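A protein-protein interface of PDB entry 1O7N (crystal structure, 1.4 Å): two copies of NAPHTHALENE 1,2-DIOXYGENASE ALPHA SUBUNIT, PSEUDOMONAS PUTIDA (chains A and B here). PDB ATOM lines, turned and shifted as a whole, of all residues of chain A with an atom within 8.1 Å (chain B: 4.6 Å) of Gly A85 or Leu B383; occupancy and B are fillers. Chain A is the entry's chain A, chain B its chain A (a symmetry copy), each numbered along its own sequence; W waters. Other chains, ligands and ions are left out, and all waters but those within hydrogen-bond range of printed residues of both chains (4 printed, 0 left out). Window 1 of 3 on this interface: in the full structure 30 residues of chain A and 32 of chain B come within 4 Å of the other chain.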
ATOM      1  N   ASN A  79     -11.875   1.819  -6.102  1.00  0.00           N
ATOM      2  CA  ASN A  79     -11.978   3.207  -6.558  1.00  0.00           C
ATOM      3  C   ASN A  79     -10.614   3.896  -6.532  1.00  0.00           C
ATOM      4  O   ASN A  79     -10.392   4.920  -5.869  1.00  0.00           O
ATOM      5  CB  ASN A  79     -12.984   3.927  -5.657  1.00  0.00           C
ATOM      6  CG  ASN A  79     -13.340   5.290  -6.158  1.00  0.00           C
ATOM      7  OD1 ASN A  79     -13.045   5.664  -7.295  1.00  0.00           O
ATOM      8  ND2 ASN A  79     -13.999   6.078  -5.305  1.00  0.00           N
ATOM      9  N   VAL A  80      -9.694   3.304  -7.287  1.00  0.00           N
ATOM     10  CA  VAL A  80      -8.286   3.711  -7.283  1.00  0.00           C
ATOM     11  C   VAL A  80      -7.734   3.592  -8.715  1.00  0.00           C
ATOM     12  O   VAL A  80      -7.817   2.520  -9.309  1.00  0.00           O
ATOM     13  CB  VAL A  80      -7.476   2.789  -6.359  1.00  0.00           C
ATOM     14  CG1 VAL A  80      -6.012   3.199  -6.354  1.00  0.00           C
ATOM     15  CG2 VAL A  80      -8.023   2.817  -4.919  1.00  0.00           C
ATOM     16  N   CYS A  81      -7.212   4.683  -9.258  1.00  0.00           N
ATOM     17  CA  CYS A  81      -6.663   4.686 -10.607  1.00  0.00           C
ATOM     18  C   CYS A  81      -5.426   3.793 -10.688  1.00  0.00           C
ATOM     19  O   CYS A  81      -4.591   3.808  -9.784  1.00  0.00           O
ATOM     20  CB  CYS A  81      -6.287   6.109 -10.960  1.00  0.00           C
ATOM     21  SG  CYS A  81      -5.675   6.221 -12.658  1.00  0.00           S
ATOM     22  N   ARG A  82      -5.301   3.042 -11.784  1.00  0.00           N
ATOM     23  CA  ARG A  82      -4.178   2.125 -11.979  1.00  0.00           C
ATOM     24  C   ARG A  82      -2.882   2.821 -12.354  1.00  0.00           C
ATOM     25  O   ARG A  82      -1.856   2.170 -12.433  1.00  0.00           O
ATOM     26  CB  ARG A  82      -4.537   1.106 -13.053  1.00  0.00           C
ATOM     27  CG  ARG A  82      -5.543   0.041 -12.619  1.00  0.00           C
ATOM     28  CD  ARG A  82      -5.038  -0.888 -11.535  1.00  0.00           C
ATOM     29  NE  ARG A  82      -3.699  -1.377 -11.780  1.00  0.00           N
ATOM     30  CZ  ARG A  82      -3.391  -2.457 -12.498  1.00  0.00           C
ATOM     31  NH1 ARG A  82      -4.338  -3.192 -13.104  1.00  0.00           N
ATOM     32  NH2 ARG A  82      -2.103  -2.792 -12.636  1.00  0.00           N
ATOM     33  N   HIS A  83      -2.906   4.116 -12.589  1.00  0.00           N
ATOM     34  CA  HIS A  83      -1.706   4.823 -12.926  1.00  0.00           C
ATOM     35  C   HIS A  83      -0.930   5.227 -11.659  1.00  0.00           C
ATOM     36  O   HIS A  83      -0.049   4.506 -11.226  1.00  0.00           O
ATOM     37  CB  HIS A  83      -2.087   6.022 -13.762  1.00  0.00           C
ATOM     38  CG  HIS A  83      -0.898   6.881 -14.191  1.00  0.00           C
ATOM     39  ND1 HIS A  83      -0.930   8.259 -14.160  1.00  0.00           N
ATOM     40  CD2 HIS A  83       0.333   6.532 -14.665  1.00  0.00           C
ATOM     41  CE1 HIS A  83       0.240   8.725 -14.590  1.00  0.00           C
ATOM     42  NE2 HIS A  83       1.017   7.697 -14.897  1.00  0.00           N
ATOM     43  N   ARG A  84      -1.251   6.393 -11.069  1.00  0.00           N
ATOM     44  CA  ARG A  84      -0.634   6.826  -9.816  1.00  0.00           C
ATOM     45  C   ARG A  84      -1.546   6.780  -8.579  1.00  0.00           C
ATOM     46  O   ARG A  84      -1.238   7.394  -7.566  1.00  0.00           O
ATOM     47  CB  ARG A  84      -0.028   8.225  -9.923  1.00  0.00           C
ATOM     48  CG  ARG A  84       0.915   8.551 -11.096  1.00  0.00           C
ATOM     49  CD  ARG A  84       2.347   7.978 -11.013  1.00  0.00           C
ATOM     50  NE  ARG A  84       3.055   8.151  -9.746  1.00  0.00           N
ATOM     51  CZ  ARG A  84       4.004   7.290  -9.376  1.00  0.00           C
ATOM     52  NH1 ARG A  84       4.301   6.270 -10.159  1.00  0.00           N
ATOM     53  NH2 ARG A  84       4.648   7.475  -8.232  1.00  0.00           N
ATOM     54  N   GLY A  85      -2.666   6.062  -8.644  1.00  0.00           N
ATOM     55  CA  GLY A  85      -3.387   5.763  -7.408  1.00  0.00           C
ATOM     56  C   GLY A  85      -4.367   6.783  -6.864  1.00  0.00           C
ATOM     57  O   GLY A  85      -4.771   6.640  -5.716  1.00  0.00           O
ATOM     58  N   LYS A  86      -4.762   7.756  -7.676  1.00  0.00           N
ATOM     59  CA  LYS A  86      -5.739   8.771  -7.264  1.00  0.00           C
ATOM     60  C   LYS A  86      -7.119   8.117  -7.126  1.00  0.00           C
ATOM     61  O   LYS A  86      -7.429   7.113  -7.770  1.00  0.00           O
ATOM     62  CB  LYS A  86      -5.784   9.829  -8.388  1.00  0.00           C
ATOM     63  CG  LYS A  86      -6.294  11.152  -7.935  1.00  0.00           C
ATOM     64  CD  LYS A  86      -7.613  11.393  -8.554  1.00  0.00           C
ATOM     65  CE  LYS A  86      -8.383  12.381  -7.713  1.00  0.00           C
ATOM     66  NZ  LYS A  86      -9.755  12.547  -8.263  1.00  0.00           N
ATOM     67  N   THR A  87      -7.963   8.676  -6.267  1.00  0.00           N
ATOM     68  CA  THR A  87      -9.319   8.150  -6.160  1.00  0.00           C
ATOM     69  C   THR A  87     -10.066   8.543  -7.433  1.00  0.00           C
ATOM     70  O   THR A  87     -10.120   9.709  -7.812  1.00  0.00           O
ATOM     71  CB  THR A  87      -9.992   8.770  -4.938  1.00  0.00           C
ATOM     72  OG1 THR A  87      -9.379   8.224  -3.762  1.00  0.00           O
ATOM     73  CG2 THR A  87     -11.490   8.372  -4.874  1.00  0.00           C
ATOM     74  N   LEU A  88     -10.669   7.562  -8.087  1.00  0.00           N
ATOM     75  CA  LEU A  88     -11.261   7.820  -9.393  1.00  0.00           C
ATOM     76  C   LEU A  88     -12.583   8.590  -9.342  1.00  0.00           C
ATOM     77  O   LEU A  88     -12.776   9.580 -10.065  1.00  0.00           O
ATOM     78  CB  LEU A  88     -11.456   6.455 -10.084  1.00  0.00           C
ATOM     79  CG  LEU A  88     -11.843   6.278 -11.552  1.00  0.00           C
ATOM     80  CD1 LEU A  88     -10.916   7.054 -12.486  1.00  0.00           C
ATOM     81  CD2 LEU A  88     -11.808   4.780 -11.918  1.00  0.00           C
ATOM     82  N   CYS A 101      -9.993   9.701 -14.775  1.00  0.00           N
ATOM     83  CA  CYS A 101      -9.211  10.164 -13.630  1.00  0.00           C
ATOM     84  C   CYS A 101      -8.845  11.624 -13.792  1.00  0.00           C
ATOM     85  O   CYS A 101      -8.357  12.041 -14.857  1.00  0.00           O
ATOM     86  CB  CYS A 101      -7.935   9.350 -13.544  1.00  0.00           C
ATOM     87  SG  CYS A 101      -6.937   9.766 -12.093  1.00  0.00           S
ATOM     88  N   TYR A 103      -6.425  13.251 -12.566  1.00  0.00           N
ATOM     89  CA  TYR A 103      -4.985  13.519 -12.480  1.00  0.00           C
ATOM     90  C   TYR A 103      -4.344  13.585 -13.898  1.00  0.00           C
ATOM     91  O   TYR A 103      -3.930  14.656 -14.333  1.00  0.00           O
ATOM     92  CB  TYR A 103      -4.297  12.485 -11.592  1.00  0.00           C
ATOM     93  CG  TYR A 103      -2.974  12.903 -10.960  1.00  0.00           C
ATOM     94  CD1 TYR A 103      -2.415  12.180  -9.910  1.00  0.00           C
ATOM     95  CD2 TYR A 103      -2.278  14.019 -11.399  1.00  0.00           C
ATOM     96  CE1 TYR A 103      -1.178  12.521  -9.369  1.00  0.00           C
ATOM     97  CE2 TYR A 103      -1.048  14.369 -10.870  1.00  0.00           C
ATOM     98  CZ  TYR A 103      -0.494  13.616  -9.856  1.00  0.00           C
ATOM     99  OH  TYR A 103       0.721  13.968  -9.315  1.00  0.00           O
ATOM    100  N   HIS A 104      -4.272  12.451 -14.586  1.00  0.00           N
ATOM    101  CA  HIS A 104      -3.729  12.416 -15.944  1.00  0.00           C
ATOM    102  C   HIS A 104      -4.753  12.016 -16.993  1.00  0.00           C
ATOM    103  O   HIS A 104      -4.406  11.848 -18.169  1.00  0.00           O
ATOM    104  CB  HIS A 104      -2.520  11.505 -16.057  1.00  0.00           C
ATOM    105  CG  HIS A 104      -1.517  11.766 -14.950  1.00  0.00           C
ATOM    106  ND1 HIS A 104      -1.620  11.130 -13.732  1.00  0.00           N
ATOM    107  CD2 HIS A 104      -0.428  12.570 -14.858  1.00  0.00           C
ATOM    108  CE1 HIS A 104      -0.646  11.528 -12.941  1.00  0.00           C
ATOM    109  NE2 HIS A 104       0.102  12.399 -13.604  1.00  0.00           N
ATOM    110  N   LEU B  14      10.513   1.597 -12.394  1.00  0.00           N
ATOM    111  CA  LEU B  14       9.330   1.471 -13.238  1.00  0.00           C
ATOM    112  C   LEU B  14       8.027   1.527 -12.448  1.00  0.00           C
ATOM    113  O   LEU B  14       6.999   1.878 -12.993  1.00  0.00           O
ATOM    114  CB  LEU B  14       9.369   0.180 -14.052  1.00  0.00           C
ATOM    115  CG  LEU B  14      10.418   0.246 -15.165  1.00  0.00           C
ATOM    116  CD1 LEU B  14      10.567  -1.117 -15.840  1.00  0.00           C
ATOM    117  CD2 LEU B  14      10.058   1.307 -16.168  1.00  0.00           C
ATOM    118  N   SER B  15       8.083   1.115 -11.185  1.00  0.00           N
ATOM    119  CA  SER B  15       6.882   1.168 -10.361  1.00  0.00           C
ATOM    120  C   SER B  15       7.277   1.267  -8.904  1.00  0.00           C
ATOM    121  O   SER B  15       8.404   0.970  -8.521  1.00  0.00           O
ATOM    122  CB  SER B  15       6.033  -0.077 -10.570  1.00  0.00           C
ATOM    123  OG  SER B  15       6.728  -1.249 -10.183  1.00  0.00           O
ATOM    124  N   GLN B  16       6.309   1.664  -8.076  1.00  0.00           N
ATOM    125  CA  GLN B  16       6.520   1.744  -6.614  1.00  0.00           C
ATOM    126  C   GLN B  16       5.314   1.161  -5.911  1.00  0.00           C
ATOM    127  O   GLN B  16       4.204   1.338  -6.374  1.00  0.00           O
ATOM    128  CB  GLN B  16       6.659   3.196  -6.143  1.00  0.00           C
ATOM    129  CG  GLN B  16       7.735   4.021  -6.917  1.00  0.00           C
ATOM    130  CD  GLN B  16       7.308   4.482  -8.281  1.00  0.00           C
ATOM    131  OE1 GLN B  16       6.220   4.987  -8.465  1.00  0.00           O
ATOM    132  NE2 GLN B  16       8.200   4.332  -9.268  1.00  0.00           N
ATOM    133  N   LYS B  17       5.535   0.532  -4.772  1.00  0.00           N
ATOM    134  CA  LYS B  17       4.398   0.057  -3.973  1.00  0.00           C
ATOM    135  C   LYS B  17       3.633   1.256  -3.434  1.00  0.00           C
ATOM    136  O   LYS B  17       4.197   2.186  -2.885  1.00  0.00           O
ATOM    137  CB  LYS B  17       4.863  -0.808  -2.800  1.00  0.00           C
ATOM    138  CG  LYS B  17       5.457  -2.183  -3.272  1.00  0.00           C
ATOM    139  CD  LYS B  17       4.398  -2.946  -4.071  1.00  0.00           C
ATOM    140  CE  LYS B  17       4.836  -4.369  -4.413  1.00  0.00           C
ATOM    141  NZ  LYS B  17       3.835  -5.072  -5.259  1.00  0.00           N
ATOM    142  N   HIS B  18       2.317   1.245  -3.585  1.00  0.00           N
ATOM    143  CA  HIS B  18       1.470   2.320  -3.123  1.00  0.00           C
ATOM    144  C   HIS B  18       1.604   2.621  -1.620  1.00  0.00           C
ATOM    145  O   HIS B  18       1.408   3.774  -1.202  1.00  0.00           O
ATOM    146  CB  HIS B  18       0.053   1.977  -3.503  1.00  0.00           C
ATOM    147  CG  HIS B  18      -0.859   3.195  -3.625  1.00  0.00           C
ATOM    148  ND1 HIS B  18      -2.062   3.120  -4.307  1.00  0.00           N
ATOM    149  CD2 HIS B  18      -0.744   4.472  -3.182  1.00  0.00           C
ATOM    150  CE1 HIS B  18      -2.662   4.297  -4.238  1.00  0.00           C
ATOM    151  NE2 HIS B  18      -1.880   5.146  -3.578  1.00  0.00           N
ATOM    152  N   HIS B  21       3.253   5.818   0.140  1.00  0.00           N
ATOM    153  CA  HIS B  21       2.612   7.097   0.480  1.00  0.00           C
ATOM    154  C   HIS B  21       1.793   7.075   1.759  1.00  0.00           C
ATOM    155  O   HIS B  21       1.307   8.155   2.188  1.00  0.00           O
ATOM    156  CB  HIS B  21       1.702   7.562  -0.651  1.00  0.00           C
ATOM    157  CG  HIS B  21       2.404   7.899  -1.922  1.00  0.00           C
ATOM    158  ND1 HIS B  21       3.679   8.409  -1.958  1.00  0.00           N
ATOM    159  CD2 HIS B  21       1.975   7.849  -3.209  1.00  0.00           C
ATOM    160  CE1 HIS B  21       4.020   8.640  -3.219  1.00  0.00           C
ATOM    161  NE2 HIS B  21       2.995   8.312  -3.992  1.00  0.00           N
ATOM    162  N   THR B 368      -5.666  12.263  -2.190  1.00  0.00           N
ATOM    163  CA  THR B 368      -6.268  10.919  -2.306  1.00  0.00           C
ATOM    164  C   THR B 368      -5.215   9.873  -2.714  1.00  0.00           C
ATOM    165  O   THR B 368      -5.262   8.751  -2.234  1.00  0.00           O
ATOM    166  CB  THR B 368      -7.503  10.881  -3.220  1.00  0.00           C
ATOM    167  OG1 THR B 368      -7.127  11.150  -4.580  1.00  0.00           O
ATOM    168  CG2 THR B 368      -8.543  11.929  -2.800  1.00  0.00           C
ATOM    169  N   ALA B 369      -4.289  10.233  -3.606  1.00  0.00           N
ATOM    170  CA  ALA B 369      -3.273   9.252  -3.956  1.00  0.00           C
ATOM    171  C   ALA B 369      -2.521   8.843  -2.686  1.00  0.00           C
ATOM    172  O   ALA B 369      -2.164   7.669  -2.546  1.00  0.00           O
ATOM    173  CB  ALA B 369      -2.322   9.797  -4.995  1.00  0.00           C
ATOM    174  N   ASN B 372      -4.883   6.745  -0.237  1.00  0.00           N
ATOM    175  CA  ASN B 372      -5.132   5.418  -0.766  1.00  0.00           C
ATOM    176  C   ASN B 372      -4.006   4.450  -0.449  1.00  0.00           C
ATOM    177  O   ASN B 372      -4.237   3.262  -0.390  1.00  0.00           O
ATOM    178  CB  ASN B 372      -5.410   5.467  -2.268  1.00  0.00           C
ATOM    179  CG  ASN B 372      -6.777   6.013  -2.580  1.00  0.00           C
ATOM    180  OD1 ASN B 372      -7.696   5.959  -1.716  1.00  0.00           O
ATOM    181  ND2 ASN B 372      -6.960   6.554  -3.776  1.00  0.00           N
ATOM    182  N   SER B 381      -0.254  -2.643  -4.080  1.00  0.00           N
ATOM    183  CA  SER B 381      -0.452  -2.359  -5.498  1.00  0.00           C
ATOM    184  C   SER B 381       0.693  -1.540  -6.046  1.00  0.00           C
ATOM    185  O   SER B 381       1.437  -0.927  -5.294  1.00  0.00           O
ATOM    186  CB  SER B 381      -1.775  -1.634  -5.750  1.00  0.00           C
ATOM    187  OG  SER B 381      -2.829  -2.499  -5.342  1.00  0.00           O
ATOM    188  N   ASP B 382       0.780  -1.441  -7.368  1.00  0.00           N
ATOM    189  CA  ASP B 382       1.933  -0.793  -8.005  1.00  0.00           C
ATOM    190  C   ASP B 382       1.567   0.500  -8.691  1.00  0.00           C
ATOM    191  O   ASP B 382       0.764   0.529  -9.624  1.00  0.00           O
ATOM    192  CB  ASP B 382       2.559  -1.756  -9.030  1.00  0.00           C
ATOM    193  CG  ASP B 382       2.933  -3.053  -8.400  1.00  0.00           C
ATOM    194  OD1 ASP B 382       3.768  -3.097  -7.471  1.00  0.00           O
ATOM    195  OD2 ASP B 382       2.385  -4.125  -8.776  1.00  0.00           O
ATOM    196  N   LEU B 383       2.162   1.582  -8.199  1.00  0.00           N
ATOM    197  CA  LEU B 383       2.083   2.861  -8.855  1.00  0.00           C
ATOM    198  C   LEU B 383       3.010   2.797 -10.079  1.00  0.00           C
ATOM    199  O   LEU B 383       4.158   2.363  -9.949  1.00  0.00           O
ATOM    200  CB  LEU B 383       2.581   3.930  -7.904  1.00  0.00           C
ATOM    201  CG  LEU B 383       1.850   4.100  -6.554  1.00  0.00           C
ATOM    202  CD1 LEU B 383       2.658   5.017  -5.625  1.00  0.00           C
ATOM    203  CD2 LEU B 383       0.436   4.673  -6.809  1.00  0.00           C
ATOM    204  N   LEU B 384       2.525   3.215 -11.242  1.00  0.00           N
ATOM    205  CA  LEU B 384       3.302   3.084 -12.486  1.00  0.00           C
ATOM    206  C   LEU B 384       4.058   4.326 -12.878  1.00  0.00           C
ATOM    207  O   LEU B 384       3.544   5.450 -12.817  1.00  0.00           O
ATOM    208  CB  LEU B 384       2.349   2.703 -13.621  1.00  0.00           C
ATOM    209  CG  LEU B 384       1.536   1.451 -13.354  1.00  0.00           C
ATOM    210  CD1 LEU B 384       0.678   1.113 -14.592  1.00  0.00           C
ATOM    211  CD2 LEU B 384       2.458   0.289 -12.944  1.00  0.00           C
ATOM    212  N   SER B 385       5.335   4.159 -13.263  1.00  0.00           N
ATOM    213  CA  SER B 385       6.096   5.279 -13.811  1.00  0.00           C
ATOM    214  C   SER B 385       6.936   4.816 -15.002  1.00  0.00           C
ATOM    215  O   SER B 385       8.149   5.022 -15.032  1.00  0.00           O
ATOM    216  CB  SER B 385       6.945   6.022 -12.780  1.00  0.00           C
ATOM    217  OG  SER B 385       7.670   5.123 -11.998  1.00  0.00           O
HETATM  218  O   HOH W   1     -10.186   4.861  -2.904  1.00  0.00           O
HETATM  219  O   HOH W   2       0.337  -4.018 -10.776  1.00  0.00           O
HETATM  220  O   HOH W   3      -0.944  -0.296 -11.519  1.00  0.00           O
HETATM  221  O   HOH W   4       1.463   8.617  -6.531  1.00  0.00           O
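Water W3 lies within hydrogen-bond range of the backbone carbonyl oxygen (O) of Asp B382 (2.7 Å) and the backbone carbonyl oxygen (O) of Arg A82 (2.8 Å). Water W2 lies within hydrogen-bond range of OD2 of Asp B382 and NH2 of Arg A82. Water W1 bridges the side-chain amide oxygen (OD1) of Asn B372 (3.0 Å) and the backbone carbonyl oxygen (O) of Asn A79 (3.0 Å). Water W4 bridges a ring nitrogen (NE2) of His B21 (3.0 Å) and the backbone carbonyl oxygen of Arg A84 (3.1 Å).
Printed residues of chain A that touch a printed residue of chain B: Arg A82, His A83, Arg A84, Gly A85, Lys A86 and Thr A87. Hydrophobic or aromatic side chains of chain A within 4 Å of the printed part of chain B: His A83. Of the 14 printed residues of chain B, 8 touch a printed residue of chain A. Along chain B the printed residues that touch a printed residue of chain A span positions 16 to 385. Among the printed residues, 16 pairs touch across the chains.
The backbone NH (N) of Leu B384 sits at hydrogen-bond distance from the backbone carbonyl oxygen (O) of His A83, 2.9 Å away. The guanidinium group (NH1) of Arg A84 is in hydrogen-bond range of the side-chain amide oxygen (OE1) of Gln B16, 2.9 Å away. The backbone carbonyl oxygen of Leu B384 lies within hydrogen-bond range of the guanidinium group of Arg A84 (2.9 Å). The backbone carbonyl oxygen (O) of Gly A85 lies within hydrogen-bond range of the side-chain amide nitrogen (ND2) of Asn B372, at 2.9 Å. N of Thr A87 is in hydrogen-bond range of OG1 of Thr B368 (3.1 Å). ND2 of Asn B372 sits at hydrogen-bond distance from OG1 of Thr A87, 2.9 Å away.
No position is printed for both chains.
O of Lys A86 sits at hydrogen-bond distance from N of Cys A81, at 2.9 Å. The backbone carbonyl oxygen (O) of Leu B14 sits at hydrogen-bond distance from the backbone NH (N) of Ser B385, 2.8 Å away. The backbone carbonyl oxygen of Gln B16 is in hydrogen-bond range of the backbone NH of Leu B383 (2.7 Å). The side-chain amide nitrogen (NE2) of Gln B16 sits at hydrogen-bond distance from the side-chain hydroxyl (OG) of Ser B385, 2.9 Å away. O of Ser B381 lies within hydrogen-bond range of N of His B18. The side-chain amide nitrogen (ND2) of Asn B372 lies close to the backbone carbonyl oxygen (O) of Thr B368, 3.2 Å away.
Of the printed residues of chain B, Arg A82 touches Leu B384 (3.5 Å). Of the printed residues of chain B, His A83 touches Leu B383 and Leu B384. Gly A85 touches just these residues of chain B: His B18, Ala B369, Asn B372 and Leu B383. Printed residues of chain B within 4 Å of Lys A86: Thr B368 and Asn B372. Of the printed residues of chain B, Thr A87 touches Thr B368 and Asn B372. Leu A88 touches none of the printed residues of chain B. Cys A101 touches none of the printed residues of chain B. Leu B383 touches just these residues of chain A: His A83 (3.6 Å), Arg A84 (3.3 Å) and Gly A85 (3.9 Å). Of the printed residues of chain A, Leu B384 touches Arg A82 (3.5 Å), His A83 (2.9 Å) and Arg A84 (2.9 Å). The nearest residue of chain B that does not touch Gly A85 is Thr B368 (4.1 Å). The nearest residue of chain A that does not touch Leu B383 is Arg A82 (5.4 Å).
Among the printed residues, merely in contact across the chains: Arg A82 with Leu B384, His A83 with Leu B383, Arg A84 with Ala B369, Arg A84 with Leu B383, Arg A84 with Ser B385, Gly A85 with His B18, Gly A85 with Ala B369, Gly A85 with Leu B383, Lys A86 with Thr B368 and Lys A86 with Asn B372.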
